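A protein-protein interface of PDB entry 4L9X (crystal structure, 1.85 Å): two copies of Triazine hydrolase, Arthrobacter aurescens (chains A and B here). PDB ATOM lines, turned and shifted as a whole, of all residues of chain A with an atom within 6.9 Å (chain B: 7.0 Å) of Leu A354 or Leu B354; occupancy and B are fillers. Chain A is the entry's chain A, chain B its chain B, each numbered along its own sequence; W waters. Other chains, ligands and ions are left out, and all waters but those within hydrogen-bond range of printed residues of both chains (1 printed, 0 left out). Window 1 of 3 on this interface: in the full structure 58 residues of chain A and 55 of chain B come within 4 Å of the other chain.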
ATOM      1  N   ILE A 310     -14.042 -18.421  -1.651  1.00  0.00           N
ATOM      2  CA  ILE A 310     -13.030 -18.612  -0.603  1.00  0.00           C
ATOM      3  C   ILE A 310     -11.665 -18.055  -1.001  1.00  0.00           C
ATOM      4  O   ILE A 310     -10.994 -17.386  -0.208  1.00  0.00           O
ATOM      5  CB  ILE A 310     -12.891 -20.107  -0.216  1.00  0.00           C
ATOM      6  CG1 ILE A 310     -11.965 -20.283   1.000  1.00  0.00           C
ATOM      7  CG2 ILE A 310     -12.385 -20.971  -1.426  1.00  0.00           C
ATOM      8  CD1 ILE A 310     -12.496 -19.635   2.310  1.00  0.00           C
ATOM      9  N   ALA A 311     -11.250 -18.328  -2.235  1.00  0.00           N
ATOM     10  CA  ALA A 311      -9.877 -18.025  -2.610  1.00  0.00           C
ATOM     11  C   ALA A 311      -9.559 -16.530  -2.516  1.00  0.00           C
ATOM     12  O   ALA A 311      -8.575 -16.161  -1.894  1.00  0.00           O
ATOM     13  CB  ALA A 311      -9.532 -18.605  -3.996  1.00  0.00           C
ATOM     14  N   PRO A 312     -10.384 -15.661  -3.131  1.00  0.00           N
ATOM     15  CA  PRO A 312     -10.082 -14.231  -2.941  1.00  0.00           C
ATOM     16  C   PRO A 312     -10.362 -13.748  -1.511  1.00  0.00           C
ATOM     17  O   PRO A 312      -9.671 -12.838  -1.054  1.00  0.00           O
ATOM     18  CB  PRO A 312     -11.031 -13.537  -3.926  1.00  0.00           C
ATOM     19  CG  PRO A 312     -12.142 -14.556  -4.173  1.00  0.00           C
ATOM     20  CD  PRO A 312     -11.448 -15.880  -4.128  1.00  0.00           C
ATOM     21  N   LEU A 314      -9.578 -15.182   1.175  1.00  0.00           N
ATOM     22  CA  LEU A 314      -8.325 -15.438   1.887  1.00  0.00           C
ATOM     23  C   LEU A 314      -7.182 -14.592   1.314  1.00  0.00           C
ATOM     24  O   LEU A 314      -6.377 -14.036   2.057  1.00  0.00           O
ATOM     25  CB  LEU A 314      -7.944 -16.920   1.803  1.00  0.00           C
ATOM     26  CG  LEU A 314      -8.915 -17.948   2.398  1.00  0.00           C
ATOM     27  CD1 LEU A 314      -8.429 -19.390   2.142  1.00  0.00           C
ATOM     28  CD2 LEU A 314      -9.117 -17.723   3.891  1.00  0.00           C
ATOM     29  N   LEU A 320     -13.337 -15.406   6.673  1.00  0.00           N
ATOM     30  CA  LEU A 320     -14.291 -16.493   6.481  1.00  0.00           C
ATOM     31  C   LEU A 320     -15.754 -16.066   6.518  1.00  0.00           C
ATOM     32  O   LEU A 320     -16.264 -15.662   7.566  1.00  0.00           O
ATOM     33  CB  LEU A 320     -14.055 -17.563   7.548  1.00  0.00           C
ATOM     34  CG  LEU A 320     -12.736 -18.336   7.501  1.00  0.00           C
ATOM     35  CD1 LEU A 320     -12.560 -19.120   8.788  1.00  0.00           C
ATOM     36  CD2 LEU A 320     -12.718 -19.269   6.312  1.00  0.00           C
ATOM     37  N   PHE A 335     -20.835 -21.272  -5.445  1.00  0.00           N
ATOM     38  CA  PHE A 335     -19.379 -21.190  -5.341  1.00  0.00           C
ATOM     39  C   PHE A 335     -18.794 -20.553  -6.595  1.00  0.00           C
ATOM     40  O   PHE A 335     -19.372 -20.660  -7.686  1.00  0.00           O
ATOM     41  CB  PHE A 335     -18.765 -22.574  -5.115  1.00  0.00           C
ATOM     42  CG  PHE A 335     -17.563 -22.557  -4.207  1.00  0.00           C
ATOM     43  CD1 PHE A 335     -16.290 -22.366  -4.724  1.00  0.00           C
ATOM     44  CD2 PHE A 335     -17.712 -22.729  -2.832  1.00  0.00           C
ATOM     45  CE1 PHE A 335     -15.176 -22.343  -3.880  1.00  0.00           C
ATOM     46  CE2 PHE A 335     -16.603 -22.714  -1.991  1.00  0.00           C
ATOM     47  CZ  PHE A 335     -15.340 -22.507  -2.522  1.00  0.00           C
ATOM     48  N   ASN A 343      -6.785 -14.980  -7.485  1.00  0.00           N
ATOM     49  CA  ASN A 343      -6.989 -16.392  -7.206  1.00  0.00           C
ATOM     50  C   ASN A 343      -5.717 -17.268  -7.081  1.00  0.00           C
ATOM     51  O   ASN A 343      -5.471 -17.806  -5.997  1.00  0.00           O
ATOM     52  CB  ASN A 343      -8.017 -16.992  -8.167  1.00  0.00           C
ATOM     53  CG  ASN A 343      -8.379 -18.400  -7.803  1.00  0.00           C
ATOM     54  OD1 ASN A 343      -7.518 -19.289  -7.799  1.00  0.00           O
ATOM     55  ND2 ASN A 343      -9.658 -18.626  -7.501  1.00  0.00           N
ATOM     56  N   LEU A 349     -12.723 -26.669  -8.472  1.00  0.00           N
ATOM     57  CA  LEU A 349     -12.628 -27.862  -7.632  1.00  0.00           C
ATOM     58  C   LEU A 349     -11.503 -27.752  -6.615  1.00  0.00           C
ATOM     59  O   LEU A 349     -11.669 -28.119  -5.456  1.00  0.00           O
ATOM     60  CB  LEU A 349     -12.436 -29.120  -8.491  1.00  0.00           C
ATOM     61  CG  LEU A 349     -12.286 -30.449  -7.753  1.00  0.00           C
ATOM     62  CD1 LEU A 349     -13.474 -30.706  -6.849  1.00  0.00           C
ATOM     63  CD2 LEU A 349     -12.094 -31.606  -8.767  1.00  0.00           C
ATOM     64  N   GLY A 350     -10.347 -27.247  -7.050  1.00  0.00           N
ATOM     65  CA  GLY A 350      -9.244 -27.029  -6.139  1.00  0.00           C
ATOM     66  C   GLY A 350      -9.629 -26.069  -5.018  1.00  0.00           C
ATOM     67  O   GLY A 350      -9.279 -26.292  -3.858  1.00  0.00           O
ATOM     68  N   ASP A 351     -10.351 -25.007  -5.351  1.00  0.00           N
ATOM     69  CA  ASP A 351     -10.722 -24.020  -4.335  1.00  0.00           C
ATOM     70  C   ASP A 351     -11.659 -24.611  -3.273  1.00  0.00           C
ATOM     71  O   ASP A 351     -11.719 -24.126  -2.139  1.00  0.00           O
ATOM     72  CB  ASP A 351     -11.378 -22.806  -4.971  1.00  0.00           C
ATOM     73  CG  ASP A 351     -10.384 -21.901  -5.713  1.00  0.00           C
ATOM     74  OD1 ASP A 351      -9.159 -22.216  -5.808  1.00  0.00           O
ATOM     75  OD2 ASP A 351     -10.874 -20.887  -6.232  1.00  0.00           O
ATOM     76  N   LEU A 352     -12.396 -25.662  -3.622  1.00  0.00           N
ATOM     77  CA  LEU A 352     -13.246 -26.308  -2.610  1.00  0.00           C
ATOM     78  C   LEU A 352     -12.432 -26.817  -1.421  1.00  0.00           C
ATOM     79  O   LEU A 352     -12.877 -26.771  -0.269  1.00  0.00           O
ATOM     80  CB  LEU A 352     -14.069 -27.456  -3.208  1.00  0.00           C
ATOM     81  CG  LEU A 352     -15.071 -27.048  -4.287  1.00  0.00           C
ATOM     82  CD1 LEU A 352     -15.916 -28.245  -4.744  1.00  0.00           C
ATOM     83  CD2 LEU A 352     -15.956 -25.928  -3.807  1.00  0.00           C
ATOM     84  N   ARG A 353     -11.241 -27.314  -1.702  1.00  0.00           N
ATOM     85  CA  ARG A 353     -10.397 -27.841  -0.650  1.00  0.00           C
ATOM     86  C   ARG A 353      -9.981 -26.725   0.292  1.00  0.00           C
ATOM     87  O   ARG A 353      -9.873 -26.946   1.478  1.00  0.00           O
ATOM     88  CB  ARG A 353      -9.167 -28.523  -1.241  1.00  0.00           C
ATOM     89  CG  ARG A 353      -8.209 -29.137  -0.233  1.00  0.00           C
ATOM     90  CD  ARG A 353      -7.081 -29.846  -1.003  1.00  0.00           C
ATOM     91  NE  ARG A 353      -5.861 -30.002  -0.233  1.00  0.00           N
ATOM     92  CZ  ARG A 353      -5.745 -30.815   0.805  1.00  0.00           C
ATOM     93  NH1 ARG A 353      -6.800 -31.539   1.197  1.00  0.00           N
ATOM     94  NH2 ARG A 353      -4.583 -30.911   1.450  1.00  0.00           N
ATOM     95  N   LEU A 354      -9.735 -25.531  -0.252  1.00  0.00           N
ATOM     96  CA  LEU A 354      -9.418 -24.364   0.569  1.00  0.00           C
ATOM     97  C   LEU A 354     -10.518 -24.093   1.578  1.00  0.00           C
ATOM     98  O   LEU A 354     -10.242 -23.810   2.744  1.00  0.00           O
ATOM     99  CB  LEU A 354      -9.259 -23.112  -0.302  1.00  0.00           C
ATOM    100  CG  LEU A 354      -8.118 -23.039  -1.312  1.00  0.00           C
ATOM    101  CD1 LEU A 354      -8.162 -21.659  -1.971  1.00  0.00           C
ATOM    102  CD2 LEU A 354      -6.764 -23.262  -0.642  1.00  0.00           C
ATOM    103  N   ALA A 355     -11.765 -24.150   1.112  1.00  0.00           N
ATOM    104  CA  ALA A 355     -12.902 -23.870   1.967  1.00  0.00           C
ATOM    105  C   ALA A 355     -13.086 -24.999   2.978  1.00  0.00           C
ATOM    106  O   ALA A 355     -13.335 -24.750   4.160  1.00  0.00           O
ATOM    107  CB  ALA A 355     -14.162 -23.682   1.128  1.00  0.00           C
ATOM    108  N   ALA A 356     -12.962 -26.239   2.511  1.00  0.00           N
ATOM    109  CA  ALA A 356     -13.050 -27.409   3.392  1.00  0.00           C
ATOM    110  C   ALA A 356     -12.131 -27.243   4.596  1.00  0.00           C
ATOM    111  O   ALA A 356     -12.525 -27.501   5.735  1.00  0.00           O
ATOM    112  CB  ALA A 356     -12.683 -28.692   2.625  1.00  0.00           C
ATOM    113  N   LEU A 357     -10.895 -26.812   4.355  1.00  0.00           N
ATOM    114  CA  LEU A 357      -9.939 -26.713   5.462  1.00  0.00           C
ATOM    115  C   LEU A 357      -9.978 -25.379   6.211  1.00  0.00           C
ATOM    116  O   LEU A 357      -9.951 -25.355   7.449  1.00  0.00           O
ATOM    117  CB  LEU A 357      -8.520 -27.032   4.972  1.00  0.00           C
ATOM    118  CG  LEU A 357      -8.327 -28.462   4.442  1.00  0.00           C
ATOM    119  CD1 LEU A 357      -6.915 -28.684   3.916  1.00  0.00           C
ATOM    120  CD2 LEU A 357      -8.647 -29.511   5.504  1.00  0.00           C
ATOM    121  N   ALA A 358     -10.056 -24.273   5.477  1.00  0.00           N
ATOM    122  CA  ALA A 358      -9.886 -22.967   6.102  1.00  0.00           C
ATOM    123  C   ALA A 358     -11.002 -22.592   7.105  1.00  0.00           C
ATOM    124  O   ALA A 358     -10.748 -21.841   8.056  1.00  0.00           O
ATOM    125  CB  ALA A 358      -9.711 -21.884   5.044  1.00  0.00           C
ATOM    126  N   HIS A 359     -12.222 -23.087   6.894  1.00  0.00           N
ATOM    127  CA  HIS A 359     -13.325 -22.805   7.825  1.00  0.00           C
ATOM    128  C   HIS A 359     -13.169 -23.443   9.214  1.00  0.00           C
ATOM    129  O   HIS A 359     -13.832 -23.027  10.179  1.00  0.00           O
ATOM    130  CB  HIS A 359     -14.675 -23.232   7.226  1.00  0.00           C
ATOM    131  CG  HIS A 359     -15.239 -22.249   6.249  1.00  0.00           C
ATOM    132  ND1 HIS A 359     -15.956 -21.138   6.644  1.00  0.00           N
ATOM    133  CD2 HIS A 359     -15.190 -22.204   4.894  1.00  0.00           C
ATOM    134  CE1 HIS A 359     -16.327 -20.453   5.573  1.00  0.00           C
ATOM    135  NE2 HIS A 359     -15.879 -21.079   4.499  1.00  0.00           N
ATOM    136  N   LEU A 376     -19.903 -28.829  -0.002  1.00  0.00           N
ATOM    137  CA  LEU A 376     -19.097 -28.011  -0.892  1.00  0.00           C
ATOM    138  C   LEU A 376     -19.354 -28.371  -2.363  1.00  0.00           C
ATOM    139  O   LEU A 376     -19.524 -27.486  -3.205  1.00  0.00           O
ATOM    140  CB  LEU A 376     -17.620 -28.185  -0.529  1.00  0.00           C
ATOM    141  CG  LEU A 376     -17.235 -27.440   0.755  1.00  0.00           C
ATOM    142  CD1 LEU A 376     -15.858 -27.898   1.245  1.00  0.00           C
ATOM    143  CD2 LEU A 376     -17.235 -25.958   0.492  1.00  0.00           C
ATOM    144  N   ILE A 425     -12.248 -33.904  -3.010  1.00  0.00           N
ATOM    145  CA  ILE A 425     -11.854 -32.683  -2.310  1.00  0.00           C
ATOM    146  C   ILE A 425     -10.547 -32.852  -1.556  1.00  0.00           C
ATOM    147  O   ILE A 425      -9.752 -31.909  -1.468  1.00  0.00           O
ATOM    148  CB  ILE A 425     -12.922 -32.259  -1.272  1.00  0.00           C
ATOM    149  CG1 ILE A 425     -14.278 -32.014  -1.950  1.00  0.00           C
ATOM    150  CG2 ILE A 425     -12.470 -31.022  -0.483  1.00  0.00           C
ATOM    151  CD1 ILE A 425     -14.225 -30.984  -3.030  1.00  0.00           C
ATOM    152  N   ILE B 310       0.695 -27.165   7.337  1.00  0.00           N
ATOM    153  CA  ILE B 310      -0.536 -26.380   7.198  1.00  0.00           C
ATOM    154  C   ILE B 310      -1.809 -27.251   7.089  1.00  0.00           C
ATOM    155  O   ILE B 310      -2.823 -26.969   7.723  1.00  0.00           O
ATOM    156  CB  ILE B 310      -0.433 -25.380   6.008  1.00  0.00           C
ATOM    157  CG1 ILE B 310      -1.574 -24.359   6.029  1.00  0.00           C
ATOM    158  CG2 ILE B 310      -0.351 -26.123   4.664  1.00  0.00           C
ATOM    159  CD1 ILE B 310      -1.558 -23.469   7.247  1.00  0.00           C
ATOM    160  N   ALA B 311      -1.751 -28.316   6.291  1.00  0.00           N
ATOM    161  CA  ALA B 311      -2.952 -29.092   6.023  1.00  0.00           C
ATOM    162  C   ALA B 311      -3.547 -29.741   7.285  1.00  0.00           C
ATOM    163  O   ALA B 311      -4.723 -29.546   7.570  1.00  0.00           O
ATOM    164  CB  ALA B 311      -2.711 -30.133   4.920  1.00  0.00           C
ATOM    165  N   PRO B 312      -2.743 -30.494   8.062  1.00  0.00           N
ATOM    166  CA  PRO B 312      -3.356 -31.050   9.281  1.00  0.00           C
ATOM    167  C   PRO B 312      -3.712 -29.971  10.310  1.00  0.00           C
ATOM    168  O   PRO B 312      -4.710 -30.142  11.014  1.00  0.00           O
ATOM    169  CB  PRO B 312      -2.274 -32.003   9.827  1.00  0.00           C
ATOM    170  CG  PRO B 312      -0.994 -31.487   9.248  1.00  0.00           C
ATOM    171  CD  PRO B 312      -1.363 -30.976   7.874  1.00  0.00           C
ATOM    172  N   LEU B 314      -4.957 -27.025   9.779  1.00  0.00           N
ATOM    173  CA  LEU B 314      -6.278 -26.542   9.404  1.00  0.00           C
ATOM    174  C   LEU B 314      -7.306 -27.650   9.583  1.00  0.00           C
ATOM    175  O   LEU B 314      -8.362 -27.428  10.171  1.00  0.00           O
ATOM    176  CB  LEU B 314      -6.300 -26.002   7.960  1.00  0.00           C
ATOM    177  CG  LEU B 314      -5.363 -24.830   7.670  1.00  0.00           C
ATOM    178  CD1 LEU B 314      -5.439 -24.411   6.174  1.00  0.00           C
ATOM    179  CD2 LEU B 314      -5.669 -23.640   8.598  1.00  0.00           C
ATOM    180  N   LEU B 320      -3.196 -21.399  12.792  1.00  0.00           N
ATOM    181  CA  LEU B 320      -1.994 -20.933  12.114  1.00  0.00           C
ATOM    182  C   LEU B 320      -0.759 -20.826  13.008  1.00  0.00           C
ATOM    183  O   LEU B 320      -0.701 -19.974  13.902  1.00  0.00           O
ATOM    184  CB  LEU B 320      -2.268 -19.560  11.497  1.00  0.00           C
ATOM    185  CG  LEU B 320      -3.368 -19.532  10.434  1.00  0.00           C
ATOM    186  CD1 LEU B 320      -3.806 -18.093  10.171  1.00  0.00           C
ATOM    187  CD2 LEU B 320      -2.882 -20.205   9.151  1.00  0.00           C
ATOM    188  N   PHE B 335       8.772 -27.877   5.519  1.00  0.00           N
ATOM    189  CA  PHE B 335       7.365 -28.122   5.215  1.00  0.00           C
ATOM    190  C   PHE B 335       7.085 -29.618   5.102  1.00  0.00           C
ATOM    191  O   PHE B 335       7.946 -30.375   4.682  1.00  0.00           O
ATOM    192  CB  PHE B 335       6.994 -27.407   3.914  1.00  0.00           C
ATOM    193  CG  PHE B 335       5.594 -26.840   3.897  1.00  0.00           C
ATOM    194  CD1 PHE B 335       5.339 -25.571   4.390  1.00  0.00           C
ATOM    195  CD2 PHE B 335       4.541 -27.572   3.367  1.00  0.00           C
ATOM    196  CE1 PHE B 335       4.050 -25.041   4.370  1.00  0.00           C
ATOM    197  CE2 PHE B 335       3.229 -27.046   3.347  1.00  0.00           C
ATOM    198  CZ  PHE B 335       2.991 -25.799   3.855  1.00  0.00           C
ATOM    199  N   ASN B 343      -4.846 -35.167   5.768  1.00  0.00           N
ATOM    200  CA  ASN B 343      -4.447 -34.265   4.696  1.00  0.00           C
ATOM    201  C   ASN B 343      -5.486 -34.029   3.577  1.00  0.00           C
ATOM    202  O   ASN B 343      -5.906 -32.892   3.392  1.00  0.00           O
ATOM    203  CB  ASN B 343      -3.084 -34.658   4.112  1.00  0.00           C
ATOM    204  CG  ASN B 343      -2.571 -33.612   3.161  1.00  0.00           C
ATOM    205  OD1 ASN B 343      -3.171 -33.385   2.115  1.00  0.00           O
ATOM    206  ND2 ASN B 343      -1.497 -32.921   3.542  1.00  0.00           N
ATOM    207  N   LEU B 349       3.317 -29.604  -2.879  1.00  0.00           N
ATOM    208  CA  LEU B 349       3.205 -28.356  -3.638  1.00  0.00           C
ATOM    209  C   LEU B 349       1.808 -27.746  -3.474  1.00  0.00           C
ATOM    210  O   LEU B 349       1.664 -26.531  -3.296  1.00  0.00           O
ATOM    211  CB  LEU B 349       3.540 -28.595  -5.125  1.00  0.00           C
ATOM    212  CG  LEU B 349       3.353 -27.393  -6.058  1.00  0.00           C
ATOM    213  CD1 LEU B 349       4.138 -26.183  -5.559  1.00  0.00           C
ATOM    214  CD2 LEU B 349       3.745 -27.747  -7.505  1.00  0.00           C
ATOM    215  N   GLY B 350       0.780 -28.596  -3.511  1.00  0.00           N
ATOM    216  CA  GLY B 350      -0.587 -28.147  -3.355  1.00  0.00           C
ATOM    217  C   GLY B 350      -0.807 -27.533  -1.979  1.00  0.00           C
ATOM    218  O   GLY B 350      -1.492 -26.524  -1.855  1.00  0.00           O
ATOM    219  N   ASP B 351      -0.207 -28.125  -0.952  1.00  0.00           N
ATOM    220  CA  ASP B 351      -0.353 -27.608   0.404  1.00  0.00           C
ATOM    221  C   ASP B 351       0.283 -26.222   0.570  1.00  0.00           C
ATOM    222  O   ASP B 351      -0.100 -25.465   1.455  1.00  0.00           O
ATOM    223  CB  ASP B 351       0.240 -28.578   1.425  1.00  0.00           C
ATOM    224  CG  ASP B 351      -0.600 -29.835   1.589  1.00  0.00           C
ATOM    225  OD1 ASP B 351      -1.711 -29.904   1.008  1.00  0.00           O
ATOM    226  OD2 ASP B 351      -0.148 -30.734   2.308  1.00  0.00           O
ATOM    227  N   LEU B 352       1.262 -25.893  -0.267  1.00  0.00           N
ATOM    228  CA  LEU B 352       1.892 -24.577  -0.182  1.00  0.00           C
ATOM    229  C   LEU B 352       0.879 -23.465  -0.462  1.00  0.00           C
ATOM    230  O   LEU B 352       0.924 -22.406   0.162  1.00  0.00           O
ATOM    231  CB  LEU B 352       3.078 -24.473  -1.147  1.00  0.00           C
ATOM    232  CG  LEU B 352       4.240 -25.438  -0.869  1.00  0.00           C
ATOM    233  CD1 LEU B 352       5.415 -25.193  -1.861  1.00  0.00           C
ATOM    234  CD2 LEU B 352       4.705 -25.325   0.587  1.00  0.00           C
ATOM    235  N   ARG B 353      -0.038 -23.711  -1.396  1.00  0.00           N
ATOM    236  CA  ARG B 353      -1.064 -22.730  -1.733  1.00  0.00           C
ATOM    237  C   ARG B 353      -2.013 -22.539  -0.546  1.00  0.00           C
ATOM    238  O   ARG B 353      -2.462 -21.438  -0.261  1.00  0.00           O
ATOM    239  CB  ARG B 353      -1.830 -23.193  -2.990  1.00  0.00           C
ATOM    240  CG  ARG B 353      -3.068 -22.378  -3.335  1.00  0.00           C
ATOM    241  CD  ARG B 353      -3.699 -22.899  -4.641  1.00  0.00           C
ATOM    242  NE  ARG B 353      -5.032 -22.349  -4.868  1.00  0.00           N
ATOM    243  CZ  ARG B 353      -5.254 -21.083  -5.196  1.00  0.00           C
ATOM    244  NH1 ARG B 353      -4.223 -20.234  -5.299  1.00  0.00           N
ATOM    245  NH2 ARG B 353      -6.494 -20.654  -5.396  1.00  0.00           N
ATOM    246  N   LEU B 354      -2.300 -23.630   0.148  1.00  0.00           N
ATOM    247  CA  LEU B 354      -3.123 -23.596   1.354  1.00  0.00           C
ATOM    248  C   LEU B 354      -2.499 -22.630   2.355  1.00  0.00           C
ATOM    249  O   LEU B 354      -3.186 -21.801   2.965  1.00  0.00           O
ATOM    250  CB  LEU B 354      -3.165 -24.998   1.957  1.00  0.00           C
ATOM    251  CG  LEU B 354      -4.434 -25.721   2.393  1.00  0.00           C
ATOM    252  CD1 LEU B 354      -5.585 -25.480   1.427  1.00  0.00           C
ATOM    253  CD2 LEU B 354      -4.111 -27.208   2.494  1.00  0.00           C
ATOM    254  N   ALA B 355      -1.188 -22.757   2.550  1.00  0.00           N
ATOM    255  CA  ALA B 355      -0.479 -21.895   3.501  1.00  0.00           C
ATOM    256  C   ALA B 355      -0.370 -20.455   2.992  1.00  0.00           C
ATOM    257  O   ALA B 355      -0.534 -19.496   3.756  1.00  0.00           O
ATOM    258  CB  ALA B 355       0.902 -22.456   3.806  1.00  0.00           C
ATOM    259  N   ALA B 356      -0.056 -20.300   1.705  1.00  0.00           N
ATOM    260  CA  ALA B 356      -0.006 -18.969   1.087  1.00  0.00           C
ATOM    261  C   ALA B 356      -1.289 -18.188   1.386  1.00  0.00           C
ATOM    262  O   ALA B 356      -1.262 -16.986   1.663  1.00  0.00           O
ATOM    263  CB  ALA B 356       0.191 -19.092  -0.446  1.00  0.00           C
ATOM    264  N   LEU B 357      -2.427 -18.871   1.304  1.00  0.00           N
ATOM    265  CA  LEU B 357      -3.695 -18.162   1.449  1.00  0.00           C
ATOM    266  C   LEU B 357      -4.189 -18.067   2.885  1.00  0.00           C
ATOM    267  O   LEU B 357      -4.656 -17.002   3.310  1.00  0.00           O
ATOM    268  CB  LEU B 357      -4.769 -18.764   0.542  1.00  0.00           C
ATOM    269  CG  LEU B 357      -4.471 -18.605  -0.954  1.00  0.00           C
ATOM    270  CD1 LEU B 357      -5.545 -19.225  -1.850  1.00  0.00           C
ATOM    271  CD2 LEU B 357      -4.315 -17.131  -1.251  1.00  0.00           C
ATOM    272  N   ALA B 358      -4.093 -19.169   3.626  1.00  0.00           N
ATOM    273  CA  ALA B 358      -4.743 -19.251   4.932  1.00  0.00           C
ATOM    274  C   ALA B 358      -4.111 -18.364   6.008  1.00  0.00           C
ATOM    275  O   ALA B 358      -4.794 -17.959   6.946  1.00  0.00           O
ATOM    276  CB  ALA B 358      -4.827 -20.687   5.405  1.00  0.00           C
ATOM    277  N   HIS B 359      -2.821 -18.062   5.884  1.00  0.00           N
ATOM    278  CA  HIS B 359      -2.167 -17.147   6.842  1.00  0.00           C
ATOM    279  C   HIS B 359      -2.615 -15.681   6.753  1.00  0.00           C
ATOM    280  O   HIS B 359      -2.438 -14.912   7.700  1.00  0.00           O
ATOM    281  CB  HIS B 359      -0.646 -17.177   6.661  1.00  0.00           C
ATOM    282  CG  HIS B 359       0.011 -18.377   7.264  1.00  0.00           C
ATOM    283  ND1 HIS B 359       0.404 -18.426   8.585  1.00  0.00           N
ATOM    284  CD2 HIS B 359       0.350 -19.575   6.727  1.00  0.00           C
ATOM    285  CE1 HIS B 359       0.951 -19.604   8.837  1.00  0.00           C
ATOM    286  NE2 HIS B 359       0.928 -20.321   7.726  1.00  0.00           N
ATOM    287  N   LEU B 376       7.687 -19.871   0.663  1.00  0.00           N
ATOM    288  CA  LEU B 376       7.031 -21.167   0.797  1.00  0.00           C
ATOM    289  C   LEU B 376       7.788 -22.241   0.001  1.00  0.00           C
ATOM    290  O   LEU B 376       8.031 -23.343   0.502  1.00  0.00           O
ATOM    291  CB  LEU B 376       5.550 -21.053   0.373  1.00  0.00           C
ATOM    292  CG  LEU B 376       4.677 -20.323   1.405  1.00  0.00           C
ATOM    293  CD1 LEU B 376       3.364 -19.804   0.798  1.00  0.00           C
ATOM    294  CD2 LEU B 376       4.409 -21.237   2.599  1.00  0.00           C
ATOM    295  N   ILE B 425       2.528 -21.659  -7.297  1.00  0.00           N
ATOM    296  CA  ILE B 425       1.718 -21.694  -6.092  1.00  0.00           C
ATOM    297  C   ILE B 425       0.288 -21.232  -6.385  1.00  0.00           C
ATOM    298  O   ILE B 425      -0.670 -21.767  -5.830  1.00  0.00           O
ATOM    299  CB  ILE B 425       2.321 -20.766  -5.003  1.00  0.00           C
ATOM    300  CG1 ILE B 425       3.744 -21.200  -4.638  1.00  0.00           C
ATOM    301  CG2 ILE B 425       1.437 -20.703  -3.750  1.00  0.00           C
ATOM    302  CD1 ILE B 425       3.919 -22.664  -4.432  1.00  0.00           C
HETATM  303  O   HOH W   1      -3.529 -28.881  -1.012  1.00  0.00           O
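Among the printed residues, pairs that only touch across the chains: Leu A354 with Leu B354, Leu A357 with Leu B354, Leu A354 with Leu B357, Leu A314 with Leu B357, Leu A357 with Leu B314, Arg A353 with Leu B354, Ala A311 with Arg B353 and Leu A354 with Arg B353.
Ala A311 touches Arg B353, but with the chains exchanged Arg A353 does not touch Ala B311 (4.02 Å). Asn A343 touches Arg B353, and with the chains exchanged Arg A353 touches Asn B343. Arg A353 touches Leu B354, and with the chains exchanged Leu A354 touches Arg B353. Leu A354 touches Leu B357, and with the chains exchanged Leu A357 touches Leu B354. Of the 12 pairs that touch across the chains among the printed residues, 11 have their exchanged pair printed and touching as well.
Of chain B, only Arg B353 (3.9 Å), Leu B354 (3.3 Å) and Leu B357 (3.6 Å) come within 4 Å of Leu A354. Of chain A, only Arg A353, Leu A354 and Leu A357 come within 4 Å of Leu B354. Printed residues of chain A within 4 Å of Asp B351: Arg A353 (3.1 Å). Printed residues of chain A within 4 Å of Leu B357: Leu A314 and Leu A354. Printed residues of chain B within 4 Å of Asp A351: Arg B353 (3.1 Å). Printed residues of chain B within 4 Å of Leu A357: Leu B314 and Leu B354. Printed residues of chain B within 4 Å of Asn A343: Arg B353 (2.8 Å). Leu A352 touches none of the printed residues of chain B. The nearest residue of chain A that does not touch Leu B354 is Leu A314 (5.8 Å). The nearest printed residue of chain B that does not touch Leu A357 is Ala B311 (4.3 Å).
O of Asn A343 is in hydrogen-bond range of NH1 of Arg B353. The guanidinium group (NH2) of Arg B353 lies within salt-bridge range of the side-chain carboxylate (OD1) of Asp A351 (3.1 Å). The guanidinium group (NH1) of Arg A353 lies within hydrogen-bond range of the backbone carbonyl oxygen (O) of Asn B343 (2.7 Å). NH2 of Arg A353 lies within salt-bridge range of OD1 of Asp B351 (3.1 Å).
Printed residues of chain A that touch a printed residue of chain B: Ala A311, Leu A314, Asn A343, Asp A351, Arg A353, Leu A354 and Leu A357. Among the printed residues, Asp or Glu carboxylates within 4 Å of a Lys or Arg side-chain nitrogen of the other chain: Asp A351 with Arg B353 (3.1 Å) and Arg A353 with Asp B351 (3.1 Å).
Water W1 lies within hydrogen-bond range of the guanidinium group (NE) of Arg A353 (2.7 Å), the side-chain carboxylate (OD1) of Asp B351 (2.9 Å) and the backbone carbonyl oxygen (O) of Gly B350 (3.2 Å).
OD2 of Asp A351 lies within hydrogen-bond range of ND2 of Asn A343 (2.9 Å). OD2 of Asp B351 sits at hydrogen-bond distance from ND2 of Asn B343, at 2.9 Å.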
